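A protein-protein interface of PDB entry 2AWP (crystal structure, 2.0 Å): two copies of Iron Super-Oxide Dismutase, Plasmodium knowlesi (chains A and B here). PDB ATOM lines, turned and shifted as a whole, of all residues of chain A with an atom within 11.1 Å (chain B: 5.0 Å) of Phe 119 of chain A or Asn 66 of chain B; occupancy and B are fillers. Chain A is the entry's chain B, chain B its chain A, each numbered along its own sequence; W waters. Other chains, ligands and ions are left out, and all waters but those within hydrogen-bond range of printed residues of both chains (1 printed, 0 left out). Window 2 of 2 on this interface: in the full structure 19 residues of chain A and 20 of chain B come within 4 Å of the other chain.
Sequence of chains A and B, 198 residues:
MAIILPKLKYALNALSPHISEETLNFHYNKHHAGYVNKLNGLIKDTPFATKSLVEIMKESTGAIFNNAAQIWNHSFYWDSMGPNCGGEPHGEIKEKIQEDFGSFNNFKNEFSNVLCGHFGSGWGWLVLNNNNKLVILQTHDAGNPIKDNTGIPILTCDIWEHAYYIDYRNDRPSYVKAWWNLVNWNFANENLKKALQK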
ATOM      1  N   SER A 112      -2.729  18.421  37.521  1.00  0.00           N
ATOM      2  CA  SER A 112      -4.001  18.067  38.131  1.00  0.00           C
ATOM      3  C   SER A 112      -5.158  18.843  37.557  1.00  0.00           C
ATOM      4  O   SER A 112      -6.215  18.260  37.323  1.00  0.00           O
ATOM      5  CB  SER A 112      -4.001  18.271  39.673  1.00  0.00           C
ATOM      6  OG  SER A 112      -3.102  17.390  40.298  1.00  0.00           O
ATOM      7  N   ASN A 113      -4.984  20.156  37.365  1.00  0.00           N
ATOM      8  CA  ASN A 113      -6.059  20.980  36.773  1.00  0.00           C
ATOM      9  C   ASN A 113      -6.449  20.467  35.401  1.00  0.00           C
ATOM     10  O   ASN A 113      -7.623  20.325  35.105  1.00  0.00           O
ATOM     11  CB  ASN A 113      -5.653  22.468  36.675  1.00  0.00           C
ATOM     12  CG  ASN A 113      -5.722  23.189  38.027  1.00  0.00           C
ATOM     13  OD1 ASN A 113      -6.121  22.601  39.031  1.00  0.00           O
ATOM     14  ND2 ASN A 113      -5.316  24.469  38.053  1.00  0.00           N
ATOM     15  N   VAL A 114      -5.443  20.213  34.574  1.00  0.00           N
ATOM     16  CA  VAL A 114      -5.658  19.721  33.228  1.00  0.00           C
ATOM     17  C   VAL A 114      -6.410  18.366  33.241  1.00  0.00           C
ATOM     18  O   VAL A 114      -7.421  18.214  32.544  1.00  0.00           O
ATOM     19  CB  VAL A 114      -4.314  19.661  32.399  1.00  0.00           C
ATOM     20  CG1 VAL A 114      -4.502  18.830  31.098  1.00  0.00           C
ATOM     21  CG2 VAL A 114      -3.804  21.091  32.054  1.00  0.00           C
ATOM     22  N   LEU A 115      -5.934  17.406  34.040  1.00  0.00           N
ATOM     23  CA  LEU A 115      -6.571  16.098  34.141  1.00  0.00           C
ATOM     24  C   LEU A 115      -8.042  16.193  34.593  1.00  0.00           C
ATOM     25  O   LEU A 115      -8.925  15.488  34.059  1.00  0.00           O
ATOM     26  CB  LEU A 115      -5.767  15.171  35.087  1.00  0.00           C
ATOM     27  CG  LEU A 115      -4.398  14.648  34.592  1.00  0.00           C
ATOM     28  CD1 LEU A 115      -3.565  13.985  35.714  1.00  0.00           C
ATOM     29  CD2 LEU A 115      -4.552  13.749  33.388  1.00  0.00           C
ATOM     30  N   CYS A 116      -8.317  17.087  35.539  1.00  0.00           N
ATOM     31  CA  CYS A 116      -9.690  17.234  36.089  1.00  0.00           C
ATOM     32  C   CYS A 116     -10.592  18.002  35.124  1.00  0.00           C
ATOM     33  O   CYS A 116     -11.813  17.815  35.117  1.00  0.00           O
ATOM     34  CB  CYS A 116      -9.663  17.926  37.470  1.00  0.00           C
ATOM     35  SG  CYS A 116      -8.840  17.000  38.830  1.00  0.00           S
ATOM     36  N   GLY A 117     -10.002  18.847  34.287  1.00  0.00           N
ATOM     37  CA  GLY A 117     -10.800  19.755  33.477  1.00  0.00           C
ATOM     38  C   GLY A 117     -11.258  19.131  32.163  1.00  0.00           C
ATOM     39  O   GLY A 117     -12.095  19.705  31.461  1.00  0.00           O
ATOM     40  N   HIS A 118     -10.711  17.958  31.809  1.00  0.00           N
ATOM     41  CA  HIS A 118     -10.922  17.446  30.459  1.00  0.00           C
ATOM     42  C   HIS A 118     -12.338  16.886  30.323  1.00  0.00           C
ATOM     43  O   HIS A 118     -12.754  16.030  31.121  1.00  0.00           O
ATOM     44  CB  HIS A 118      -9.873  16.388  30.049  1.00  0.00           C
ATOM     45  CG  HIS A 118      -9.944  16.014  28.600  1.00  0.00           C
ATOM     46  ND1 HIS A 118      -9.179  16.631  27.635  1.00  0.00           N
ATOM     47  CD2 HIS A 118     -10.695  15.086  27.951  1.00  0.00           C
ATOM     48  CE1 HIS A 118      -9.462  16.109  26.451  1.00  0.00           C
ATOM     49  NE2 HIS A 118     -10.391  15.179  26.615  1.00  0.00           N
ATOM     50  N   PHE A 119     -13.052  17.383  29.313  1.00  0.00           N
ATOM     51  CA  PHE A 119     -14.445  17.002  29.069  1.00  0.00           C
ATOM     52  C   PHE A 119     -14.518  15.771  28.176  1.00  0.00           C
ATOM     53  O   PHE A 119     -13.918  15.758  27.103  1.00  0.00           O
ATOM     54  CB  PHE A 119     -15.241  18.152  28.425  1.00  0.00           C
ATOM     55  CG  PHE A 119     -16.699  17.835  28.253  1.00  0.00           C
ATOM     56  CD1 PHE A 119     -17.538  17.789  29.353  1.00  0.00           C
ATOM     57  CD2 PHE A 119     -17.223  17.534  27.000  1.00  0.00           C
ATOM     58  CE1 PHE A 119     -18.881  17.471  29.223  1.00  0.00           C
ATOM     59  CE2 PHE A 119     -18.583  17.222  26.857  1.00  0.00           C
ATOM     60  CZ  PHE A 119     -19.404  17.186  27.977  1.00  0.00           C
ATOM     61  N   GLY A 120     -15.271  14.772  28.620  1.00  0.00           N
ATOM     62  CA  GLY A 120     -15.433  13.508  27.890  1.00  0.00           C
ATOM     63  C   GLY A 120     -14.226  12.628  28.129  1.00  0.00           C
ATOM     64  O   GLY A 120     -13.493  12.824  29.115  1.00  0.00           O
ATOM     65  N   SER A 121     -13.999  11.687  27.208  1.00  0.00           N
ATOM     66  CA  SER A 121     -12.904  10.719  27.342  1.00  0.00           C
ATOM     67  C   SER A 121     -11.613  11.330  26.821  1.00  0.00           C
ATOM     68  O   SER A 121     -11.626  12.037  25.796  1.00  0.00           O
ATOM     69  CB  SER A 121     -13.262   9.441  26.566  1.00  0.00           C
ATOM     70  OG  SER A 121     -14.539   8.951  26.977  1.00  0.00           O
ATOM     71  N   GLY A 122     -10.513  11.076  27.529  1.00  0.00           N
ATOM     72  CA  GLY A 122      -9.177  11.456  27.087  1.00  0.00           C
ATOM     73  C   GLY A 122      -8.027  11.186  28.053  1.00  0.00           C
ATOM     74  O   GLY A 122      -8.102  10.326  28.981  1.00  0.00           O
ATOM     75  N   TRP A 123      -6.970  11.967  27.864  1.00  0.00           N
ATOM     76  CA  TRP A 123      -5.665  11.698  28.455  1.00  0.00           C
ATOM     77  C   TRP A 123      -4.954  13.012  28.748  1.00  0.00           C
ATOM     78  O   TRP A 123      -4.988  13.955  27.932  1.00  0.00           O
ATOM     79  CB  TRP A 123      -4.791  10.913  27.469  1.00  0.00           C
ATOM     80  CG  TRP A 123      -5.325   9.581  27.043  1.00  0.00           C
ATOM     81  CD1 TRP A 123      -6.251   9.333  26.063  1.00  0.00           C
ATOM     82  CD2 TRP A 123      -4.976   8.297  27.598  1.00  0.00           C
ATOM     83  NE1 TRP A 123      -6.492   7.983  25.963  1.00  0.00           N
ATOM     84  CE2 TRP A 123      -5.710   7.318  26.876  1.00  0.00           C
ATOM     85  CE3 TRP A 123      -4.083   7.882  28.604  1.00  0.00           C
ATOM     86  CZ2 TRP A 123      -5.635   5.956  27.174  1.00  0.00           C
ATOM     87  CZ3 TRP A 123      -3.993   6.506  28.902  1.00  0.00           C
ATOM     88  CH2 TRP A 123      -4.753   5.566  28.173  1.00  0.00           C
ATOM     89  N   GLY A 124      -4.266  13.070  29.895  1.00  0.00           N
ATOM     90  CA  GLY A 124      -3.254  14.111  30.130  1.00  0.00           C
ATOM     91  C   GLY A 124      -1.843  13.597  29.862  1.00  0.00           C
ATOM     92  O   GLY A 124      -1.542  12.412  30.114  1.00  0.00           O
ATOM     93  N   GLN A 138      -3.106  17.807  26.705  1.00  0.00           N
ATOM     94  CA  GLN A 138      -4.254  16.911  26.804  1.00  0.00           C
ATOM     95  C   GLN A 138      -4.697  16.490  25.412  1.00  0.00           C
ATOM     96  O   GLN A 138      -4.576  17.250  24.411  1.00  0.00           O
ATOM     97  CB  GLN A 138      -5.409  17.536  27.606  1.00  0.00           C
ATOM     98  CG  GLN A 138      -6.018  18.775  26.953  1.00  0.00           C
ATOM     99  CD  GLN A 138      -7.003  19.500  27.826  1.00  0.00           C
ATOM    100  OE1 GLN A 138      -7.920  18.898  28.403  1.00  0.00           O
ATOM    101  NE2 GLN A 138      -6.826  20.820  27.931  1.00  0.00           N
ATOM    102  N   THR A 139      -5.193  15.268  25.327  1.00  0.00           N
ATOM    103  CA  THR A 139      -5.750  14.784  24.069  1.00  0.00           C
ATOM    104  C   THR A 139      -7.103  14.158  24.350  1.00  0.00           C
ATOM    105  O   THR A 139      -7.410  13.792  25.490  1.00  0.00           O
ATOM    106  CB  THR A 139      -4.826  13.755  23.356  1.00  0.00           C
ATOM    107  OG1 THR A 139      -4.718  12.578  24.178  1.00  0.00           O
ATOM    108  CG2 THR A 139      -3.440  14.347  23.094  1.00  0.00           C
ATOM    109  N   HIS A 140      -7.910  14.039  23.299  1.00  0.00           N
ATOM    110  CA  HIS A 140      -9.271  13.553  23.413  1.00  0.00           C
ATOM    111  C   HIS A 140      -9.325  12.121  22.881  1.00  0.00           C
ATOM    112  O   HIS A 140      -8.590  11.765  21.953  1.00  0.00           O
ATOM    113  CB  HIS A 140     -10.195  14.499  22.636  1.00  0.00           C
ATOM    114  CG  HIS A 140     -11.629  14.407  23.028  1.00  0.00           C
ATOM    115  ND1 HIS A 140     -12.062  14.582  24.331  1.00  0.00           N
ATOM    116  CD2 HIS A 140     -12.739  14.186  22.284  1.00  0.00           C
ATOM    117  CE1 HIS A 140     -13.374  14.437  24.374  1.00  0.00           C
ATOM    118  NE2 HIS A 140     -13.808  14.203  23.147  1.00  0.00           N
ATOM    119  N   ASP A 141     -10.176  11.300  23.496  1.00  0.00           N
ATOM    120  CA  ASP A 141     -10.456   9.936  23.054  1.00  0.00           C
ATOM    121  C   ASP A 141      -9.183   9.091  22.973  1.00  0.00           C
ATOM    122  O   ASP A 141      -8.562   8.874  24.027  1.00  0.00           O
ATOM    123  CB  ASP A 141     -11.280   9.926  21.753  1.00  0.00           C
ATOM    124  CG  ASP A 141     -12.605  10.641  21.919  1.00  0.00           C
ATOM    125  OD1 ASP A 141     -13.208  10.476  22.980  1.00  0.00           O
ATOM    126  OD2 ASP A 141     -13.043  11.379  21.007  1.00  0.00           O
ATOM    127  N   ALA A 142      -8.791   8.637  21.768  1.00  0.00           N
ATOM    128  CA  ALA A 142      -7.528   7.841  21.572  1.00  0.00           C
ATOM    129  C   ALA A 142      -6.301   8.677  21.128  1.00  0.00           C
ATOM    130  O   ALA A 142      -5.174   8.145  20.961  1.00  0.00           O
ATOM    131  CB  ALA A 142      -7.772   6.682  20.606  1.00  0.00           C
ATOM    132  N   ASP A 158      -4.624   8.401  32.163  1.00  0.00           N
ATOM    133  CA  ASP A 158      -5.933   8.151  31.582  1.00  0.00           C
ATOM    134  C   ASP A 158      -7.062   8.773  32.411  1.00  0.00           C
ATOM    135  O   ASP A 158      -7.150   8.524  33.632  1.00  0.00           O
ATOM    136  CB  ASP A 158      -6.072   6.644  31.525  1.00  0.00           C
ATOM    137  CG  ASP A 158      -7.260   6.183  30.754  1.00  0.00           C
ATOM    138  OD1 ASP A 158      -7.940   6.930  30.050  1.00  0.00           O
ATOM    139  OD2 ASP A 158      -7.493   5.016  30.892  1.00  0.00           O
ATOM    140  N   ILE A 159      -7.910   9.592  31.766  1.00  0.00           N
ATOM    141  CA  ILE A 159      -9.103  10.119  32.425  1.00  0.00           C
ATOM    142  C   ILE A 159     -10.448   9.678  31.810  1.00  0.00           C
ATOM    143  O   ILE A 159     -11.481  10.205  32.158  1.00  0.00           O
ATOM    144  CB  ILE A 159      -9.038  11.676  32.742  1.00  0.00           C
ATOM    145  CG1 ILE A 159      -8.680  12.515  31.507  1.00  0.00           C
ATOM    146  CG2 ILE A 159      -8.065  11.946  33.911  1.00  0.00           C
ATOM    147  CD1 ILE A 159      -9.879  12.776  30.576  1.00  0.00           C
ATOM    148  N   TRP A 160     -10.423   8.681  30.935  1.00  0.00           N
ATOM    149  CA  TRP A 160     -11.646   7.959  30.619  1.00  0.00           C
ATOM    150  C   TRP A 160     -12.296   7.524  31.925  1.00  0.00           C
ATOM    151  O   TRP A 160     -11.603   7.136  32.868  1.00  0.00           O
ATOM    152  CB  TRP A 160     -11.304   6.715  29.825  1.00  0.00           C
ATOM    153  CG  TRP A 160     -11.009   6.945  28.370  1.00  0.00           C
ATOM    154  CD1 TRP A 160      -9.971   7.643  27.841  1.00  0.00           C
ATOM    155  CD2 TRP A 160     -11.736   6.388  27.250  1.00  0.00           C
ATOM    156  NE1 TRP A 160     -10.016   7.587  26.445  1.00  0.00           N
ATOM    157  CE2 TRP A 160     -11.087   6.820  26.061  1.00  0.00           C
ATOM    158  CE3 TRP A 160     -12.882   5.572  27.137  1.00  0.00           C
ATOM    159  CZ2 TRP A 160     -11.554   6.476  24.771  1.00  0.00           C
ATOM    160  CZ3 TRP A 160     -13.348   5.232  25.850  1.00  0.00           C
ATOM    161  CH2 TRP A 160     -12.679   5.679  24.692  1.00  0.00           C
ATOM    162  N   GLU A 161     -13.627   7.544  31.945  1.00  0.00           N
ATOM    163  CA  GLU A 161     -14.388   7.157  33.125  1.00  0.00           C
ATOM    164  C   GLU A 161     -14.112   5.758  33.631  1.00  0.00           C
ATOM    165  O   GLU A 161     -14.060   5.576  34.832  1.00  0.00           O
ATOM    166  CB  GLU A 161     -15.886   7.398  32.915  1.00  0.00           C
ATOM    167  CG  GLU A 161     -16.182   8.883  32.893  1.00  0.00           C
ATOM    168  CD  GLU A 161     -17.639   9.215  32.630  1.00  0.00           C
ATOM    169  OE1 GLU A 161     -18.302   8.487  31.866  1.00  0.00           O
ATOM    170  OE2 GLU A 161     -18.088  10.238  33.168  1.00  0.00           O
ATOM    171  N   TYR A 164     -11.481   5.145  36.547  1.00  0.00           N
ATOM    172  CA  TYR A 164     -11.697   5.507  37.949  1.00  0.00           C
ATOM    173  C   TYR A 164     -13.093   5.185  38.497  1.00  0.00           C
ATOM    174  O   TYR A 164     -13.279   5.144  39.742  1.00  0.00           O
ATOM    175  CB  TYR A 164     -11.330   6.978  38.176  1.00  0.00           C
ATOM    176  CG  TYR A 164     -12.103   7.992  37.339  1.00  0.00           C
ATOM    177  CD1 TYR A 164     -13.327   8.512  37.789  1.00  0.00           C
ATOM    178  CD2 TYR A 164     -11.603   8.437  36.108  1.00  0.00           C
ATOM    179  CE1 TYR A 164     -14.052   9.451  37.027  1.00  0.00           C
ATOM    180  CE2 TYR A 164     -12.288   9.410  35.344  1.00  0.00           C
ATOM    181  CZ  TYR A 164     -13.526   9.901  35.803  1.00  0.00           C
ATOM    182  OH  TYR A 164     -14.225  10.846  35.048  1.00  0.00           O
ATOM    183  N   ARG A 172     -13.657  12.277  39.849  1.00  0.00           N
ATOM    184  CA  ARG A 172     -12.395  12.253  39.135  1.00  0.00           C
ATOM    185  C   ARG A 172     -11.244  12.947  39.903  1.00  0.00           C
ATOM    186  O   ARG A 172     -10.089  12.477  39.825  1.00  0.00           O
ATOM    187  CB  ARG A 172     -12.524  12.847  37.726  1.00  0.00           C
ATOM    188  CG  ARG A 172     -11.277  12.563  36.861  1.00  0.00           C
ATOM    189  CD  ARG A 172     -11.179  13.464  35.646  1.00  0.00           C
ATOM    190  NE  ARG A 172     -12.226  13.179  34.671  1.00  0.00           N
ATOM    191  CZ  ARG A 172     -12.417  13.867  33.552  1.00  0.00           C
ATOM    192  NH1 ARG A 172     -11.614  14.880  33.263  1.00  0.00           N
ATOM    193  NH2 ARG A 172     -13.407  13.541  32.727  1.00  0.00           N
ATOM    194  N   TYR B  35     -23.879  19.480  35.837  1.00  0.00           N
ATOM    195  CA  TYR B  35     -23.901  20.273  34.607  1.00  0.00           C
ATOM    196  C   TYR B  35     -24.759  21.547  34.758  1.00  0.00           C
ATOM    197  O   TYR B  35     -24.390  22.592  34.231  1.00  0.00           O
ATOM    198  CB  TYR B  35     -24.464  19.479  33.449  1.00  0.00           C
ATOM    199  CG  TYR B  35     -23.628  18.287  32.989  1.00  0.00           C
ATOM    200  CD1 TYR B  35     -22.331  18.466  32.504  1.00  0.00           C
ATOM    201  CD2 TYR B  35     -24.182  17.011  32.956  1.00  0.00           C
ATOM    202  CE1 TYR B  35     -21.565  17.388  32.051  1.00  0.00           C
ATOM    203  CE2 TYR B  35     -23.429  15.897  32.502  1.00  0.00           C
ATOM    204  CZ  TYR B  35     -22.135  16.095  32.044  1.00  0.00           C
ATOM    205  OH  TYR B  35     -21.408  15.011  31.590  1.00  0.00           O
ATOM    206  N   GLY B  62     -17.692  25.662  23.303  1.00  0.00           N
ATOM    207  CA  GLY B  62     -16.805  25.499  24.457  1.00  0.00           C
ATOM    208  C   GLY B  62     -17.508  24.917  25.681  1.00  0.00           C
ATOM    209  O   GLY B  62     -18.443  24.122  25.546  1.00  0.00           O
ATOM    210  N   ALA B  63     -17.060  25.307  26.874  1.00  0.00           N
ATOM    211  CA  ALA B  63     -17.614  24.799  28.117  1.00  0.00           C
ATOM    212  C   ALA B  63     -19.098  25.079  28.328  1.00  0.00           C
ATOM    213  O   ALA B  63     -19.814  24.241  28.902  1.00  0.00           O
ATOM    214  CB  ALA B  63     -16.795  25.286  29.338  1.00  0.00           C
ATOM    215  N   ILE B  64     -19.551  26.256  27.888  1.00  0.00           N
ATOM    216  CA  ILE B  64     -20.978  26.641  28.010  1.00  0.00           C
ATOM    217  C   ILE B  64     -21.831  25.667  27.218  1.00  0.00           C
ATOM    218  O   ILE B  64     -22.787  25.118  27.738  1.00  0.00           O
ATOM    219  CB  ILE B  64     -21.264  28.133  27.591  1.00  0.00           C
ATOM    220  CG1 ILE B  64     -20.681  29.105  28.615  1.00  0.00           C
ATOM    221  CG2 ILE B  64     -22.794  28.396  27.486  1.00  0.00           C
ATOM    222  CD1 ILE B  64     -20.587  30.576  28.034  1.00  0.00           C
ATOM    223  N   PHE B  65     -21.421  25.400  25.983  1.00  0.00           N
ATOM    224  CA  PHE B  65     -22.139  24.432  25.168  1.00  0.00           C
ATOM    225  C   PHE B  65     -22.130  23.058  25.814  1.00  0.00           C
ATOM    226  O   PHE B  65     -23.183  22.410  25.945  1.00  0.00           O
ATOM    227  CB  PHE B  65     -21.598  24.340  23.739  1.00  0.00           C
ATOM    228  CG  PHE B  65     -22.238  23.230  22.941  1.00  0.00           C
ATOM    229  CD1 PHE B  65     -23.490  23.421  22.346  1.00  0.00           C
ATOM    230  CD2 PHE B  65     -21.624  21.975  22.851  1.00  0.00           C
ATOM    231  CE1 PHE B  65     -24.103  22.385  21.654  1.00  0.00           C
ATOM    232  CE2 PHE B  65     -22.218  20.932  22.143  1.00  0.00           C
ATOM    233  CZ  PHE B  65     -23.446  21.130  21.546  1.00  0.00           C
ATOM    234  N   ASN B  66     -20.944  22.612  26.219  1.00  0.00           N
ATOM    235  CA  ASN B  66     -20.805  21.273  26.781  1.00  0.00           C
ATOM    236  C   ASN B  66     -21.775  21.074  27.951  1.00  0.00           C
ATOM    237  O   ASN B  66     -22.514  20.089  27.987  1.00  0.00           O
ATOM    238  CB  ASN B  66     -19.361  21.019  27.224  1.00  0.00           C
ATOM    239  CG  ASN B  66     -18.408  20.808  26.046  1.00  0.00           C
ATOM    240  OD1 ASN B  66     -18.818  20.532  24.911  1.00  0.00           O
ATOM    241  ND2 ASN B  66     -17.131  20.934  26.322  1.00  0.00           N
ATOM    242  N   ASN B  67     -21.792  22.032  28.885  1.00  0.00           N
ATOM    243  CA  ASN B  67     -22.702  21.954  30.017  1.00  0.00           C
ATOM    244  C   ASN B  67     -24.176  22.097  29.647  1.00  0.00           C
ATOM    245  O   ASN B  67     -24.979  21.268  30.044  1.00  0.00           O
ATOM    246  CB  ASN B  67     -22.301  22.924  31.127  1.00  0.00           C
ATOM    247  CG  ASN B  67     -21.063  22.477  31.821  1.00  0.00           C
ATOM    248  OD1 ASN B  67     -21.115  21.592  32.698  1.00  0.00           O
ATOM    249  ND2 ASN B  67     -19.902  23.008  31.367  1.00  0.00           N
ATOM    250  N   ALA B  68     -24.516  23.144  28.897  1.00  0.00           N
ATOM    251  CA  ALA B  68     -25.904  23.333  28.392  1.00  0.00           C
ATOM    252  C   ALA B  68     -26.443  22.103  27.638  1.00  0.00           C
ATOM    253  O   ALA B  68     -27.547  21.640  27.899  1.00  0.00           O
ATOM    254  CB  ALA B  68     -25.977  24.549  27.492  1.00  0.00           C
ATOM    255  N   ALA B  69     -25.679  21.599  26.683  1.00  0.00           N
ATOM    256  CA  ALA B  69     -26.149  20.459  25.873  1.00  0.00           C
ATOM    257  C   ALA B  69     -26.275  19.200  26.742  1.00  0.00           C
ATOM    258  O   ALA B  69     -27.246  18.459  26.631  1.00  0.00           O
ATOM    259  CB  ALA B  69     -25.217  20.224  24.699  1.00  0.00           C
ATOM    260  N   GLN B  70     -25.326  18.979  27.657  1.00  0.00           N
ATOM    261  CA  GLN B  70     -25.487  17.862  28.574  1.00  0.00           C
ATOM    262  C   GLN B  70     -26.733  17.955  29.455  1.00  0.00           C
ATOM    263  O   GLN B  70     -27.386  16.934  29.710  1.00  0.00           O
ATOM    264  CB  GLN B  70     -24.239  17.619  29.417  1.00  0.00           C
ATOM    265  CG  GLN B  70     -23.065  17.036  28.625  1.00  0.00           C
ATOM    266  CD  GLN B  70     -23.283  15.641  28.146  1.00  0.00           C
ATOM    267  OE1 GLN B  70     -23.938  15.425  27.131  1.00  0.00           O
ATOM    268  NE2 GLN B  70     -22.686  14.657  28.855  1.00  0.00           N
ATOM    269  N   ASP B 141     -19.665  13.084  22.736  1.00  0.00           N
ATOM    270  CA  ASP B 141     -19.586  13.938  23.929  1.00  0.00           C
ATOM    271  C   ASP B 141     -20.949  14.591  24.274  1.00  0.00           C
ATOM    272  O   ASP B 141     -21.866  13.875  24.677  1.00  0.00           O
ATOM    273  CB  ASP B 141     -18.437  14.956  23.760  1.00  0.00           C
ATOM    274  CG  ASP B 141     -17.090  14.276  23.561  1.00  0.00           C
ATOM    275  OD1 ASP B 141     -16.774  13.304  24.254  1.00  0.00           O
ATOM    276  OD2 ASP B 141     -16.328  14.717  22.711  1.00  0.00           O
ATOM    277  N   ALA B 142     -21.073  15.913  24.142  1.00  0.00           N
ATOM    278  CA  ALA B 142     -22.320  16.657  24.448  1.00  0.00           C
ATOM    279  C   ALA B 142     -23.156  16.974  23.198  1.00  0.00           C
ATOM    280  O   ALA B 142     -24.209  17.642  23.276  1.00  0.00           O
ATOM    281  CB  ALA B 142     -22.005  17.938  25.182  1.00  0.00           C
ATOM    282  N   TRP B 160     -22.177   7.367  27.395  1.00  0.00           N
ATOM    283  CA  TRP B 160     -21.046   7.705  28.299  1.00  0.00           C
ATOM    284  C   TRP B 160     -20.891   6.549  29.300  1.00  0.00           C
ATOM    285  O   TRP B 160     -21.894   5.975  29.749  1.00  0.00           O
ATOM    286  CB  TRP B 160     -21.275   8.985  29.083  1.00  0.00           C
ATOM    287  CG  TRP B 160     -21.105  10.313  28.325  1.00  0.00           C
ATOM    288  CD1 TRP B 160     -21.774  10.718  27.206  1.00  0.00           C
ATOM    289  CD2 TRP B 160     -20.272  11.416  28.709  1.00  0.00           C
ATOM    290  NE1 TRP B 160     -21.383  11.988  26.852  1.00  0.00           N
ATOM    291  CE2 TRP B 160     -20.469  12.441  27.760  1.00  0.00           C
ATOM    292  CE3 TRP B 160     -19.326  11.608  29.723  1.00  0.00           C
ATOM    293  CZ2 TRP B 160     -19.754  13.645  27.797  1.00  0.00           C
ATOM    294  CZ3 TRP B 160     -18.637  12.798  29.775  1.00  0.00           C
ATOM    295  CH2 TRP B 160     -18.875  13.825  28.844  1.00  0.00           C
HETATM  296  O   HOH W   1     -15.216  11.241  24.543  1.00  0.00           O
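Water W1 lies within hydrogen-bond range of the side-chain carboxylate (OD1) of Asp 141 of chain B, the side-chain carboxylate (OD1) of Asp 141 of chain A and the backbone NH (N) of Ser 121 of chain A.
OD2 of Asp 141 of chain B lies within hydrogen-bond range of NE2 of His 140 of chain A.
Of the 13 printed residues of chain B, 6 touch a printed residue of chain A.
Hydrophobic or aromatic side chains of chain B within 4 Å of the printed part of chain A: Tyr 35, Ala 142 and Trp 160.
Printed residues of chain A that touch a printed residue of chain B: Phe 119, Gly 120, His 140 and Glu 161.
Hydrophobic or aromatic side chains of chain A that line the printed part of chain B: Phe 119 and His 140.
CE1 of Phe 119 of chain A touches CE1 of Tyr 35 of chain B, at 3.9 Å.
Asn 66 of chain B touches Phe 119 of chain A (ND2 to CD2, 3.5 Å).
CG of Gln 70 of chain B touches CZ of Phe 119 of chain A, 3.7 Å away.
Phe 119 of chain A touches Asp 141 of chain B (CE2 to CB, 3.8 Å).
CE2 of Phe 119 of chain A touches CB of Ala 142 of chain B, 3.9 Å away.
CZ of Phe 119 of chain A touches CH2 of Trp 160 of chain B, 3.5 Å away.
CA of Gly 120 of chain A touches OD1 of Asp 141 of chain B (3.9 Å).
Trp 160 of chain B touches Gly 120 of chain A (CH2 to CA, 3.6 Å).
Glu 161 of chain A touches Trp 160 of chain B.
3 positions are printed for both chains.
Of the 10 pairs that touch across the chains among the printed residues, none has its exchanged pair printed and touching as well.
Printed residues of chain B within 4 Å of Phe 119 of chain A: Tyr 35 (3.9 Å), Asn 66 (3.5 Å), Gln 70 (3.7 Å), Asp 141 (3.8 Å), Ala 142 (3.9 Å) and Trp 160 (3.5 Å).
Asn 66 of chain B touches just one residue of chain A: Phe 119.
No residue of chain A comes within 4 Å of Ala 63 of chain B.
No residue of chain A comes within 4 Å of Phe 65 of chain B.
No residue of chain A comes within 4 Å of Asn 67 of chain B.
No residue of chain A comes within 4 Å of Ala 69 of chain B.
Asp 141 of chain B touches just these residues of chain A: Phe 119 (3.8 Å), Gly 120 (3.9 Å) and His 140 (2.6 Å).
Of chain A, only Phe 119 (3.9 Å) comes within 4 Å of Ala 142 of chain B.
Of the printed residues of chain A, Tyr 35 of chain B touches Phe 119.
Of the printed residues of chain B, Gly 120 of chain A touches Asp 141 and Trp 160.
Of the printed residues of chain B, Glu 161 of chain A touches Trp 160 (3.9 Å).
Of the printed residues of chain B, His 140 of chain A touches Asp 141 (2.6 Å).
Printed residues of chain A within 4 Å of Trp 160 of chain B: Phe 119 (3.5 Å), Gly 120 (3.6 Å) and Glu 161 (3.9 Å).
Ser 121 of chain A touches none of the printed residues of chain B.
Thr 139 of chain A touches none of the printed residues of chain B.
The side-chain amide nitrogen (NE2) of Gln 70 of chain B sits at hydrogen-bond distance from the side-chain hydroxyl (OH) of Tyr 35 of chain B (3.0 Å).
The backbone carbonyl oxygen (O) of Asp 141 of chain B sits at hydrogen-bond distance from the indole nitrogen (NE1) of Trp 160 of chain B (2.9 Å).
NE2 of His 118 of chain A is in hydrogen-bond range of ND1 of His 140 of chain A (2.9 Å).
O of Ser 121 of chain A is in hydrogen-bond range of ND1 of His 140 of chain A (3.0 Å).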
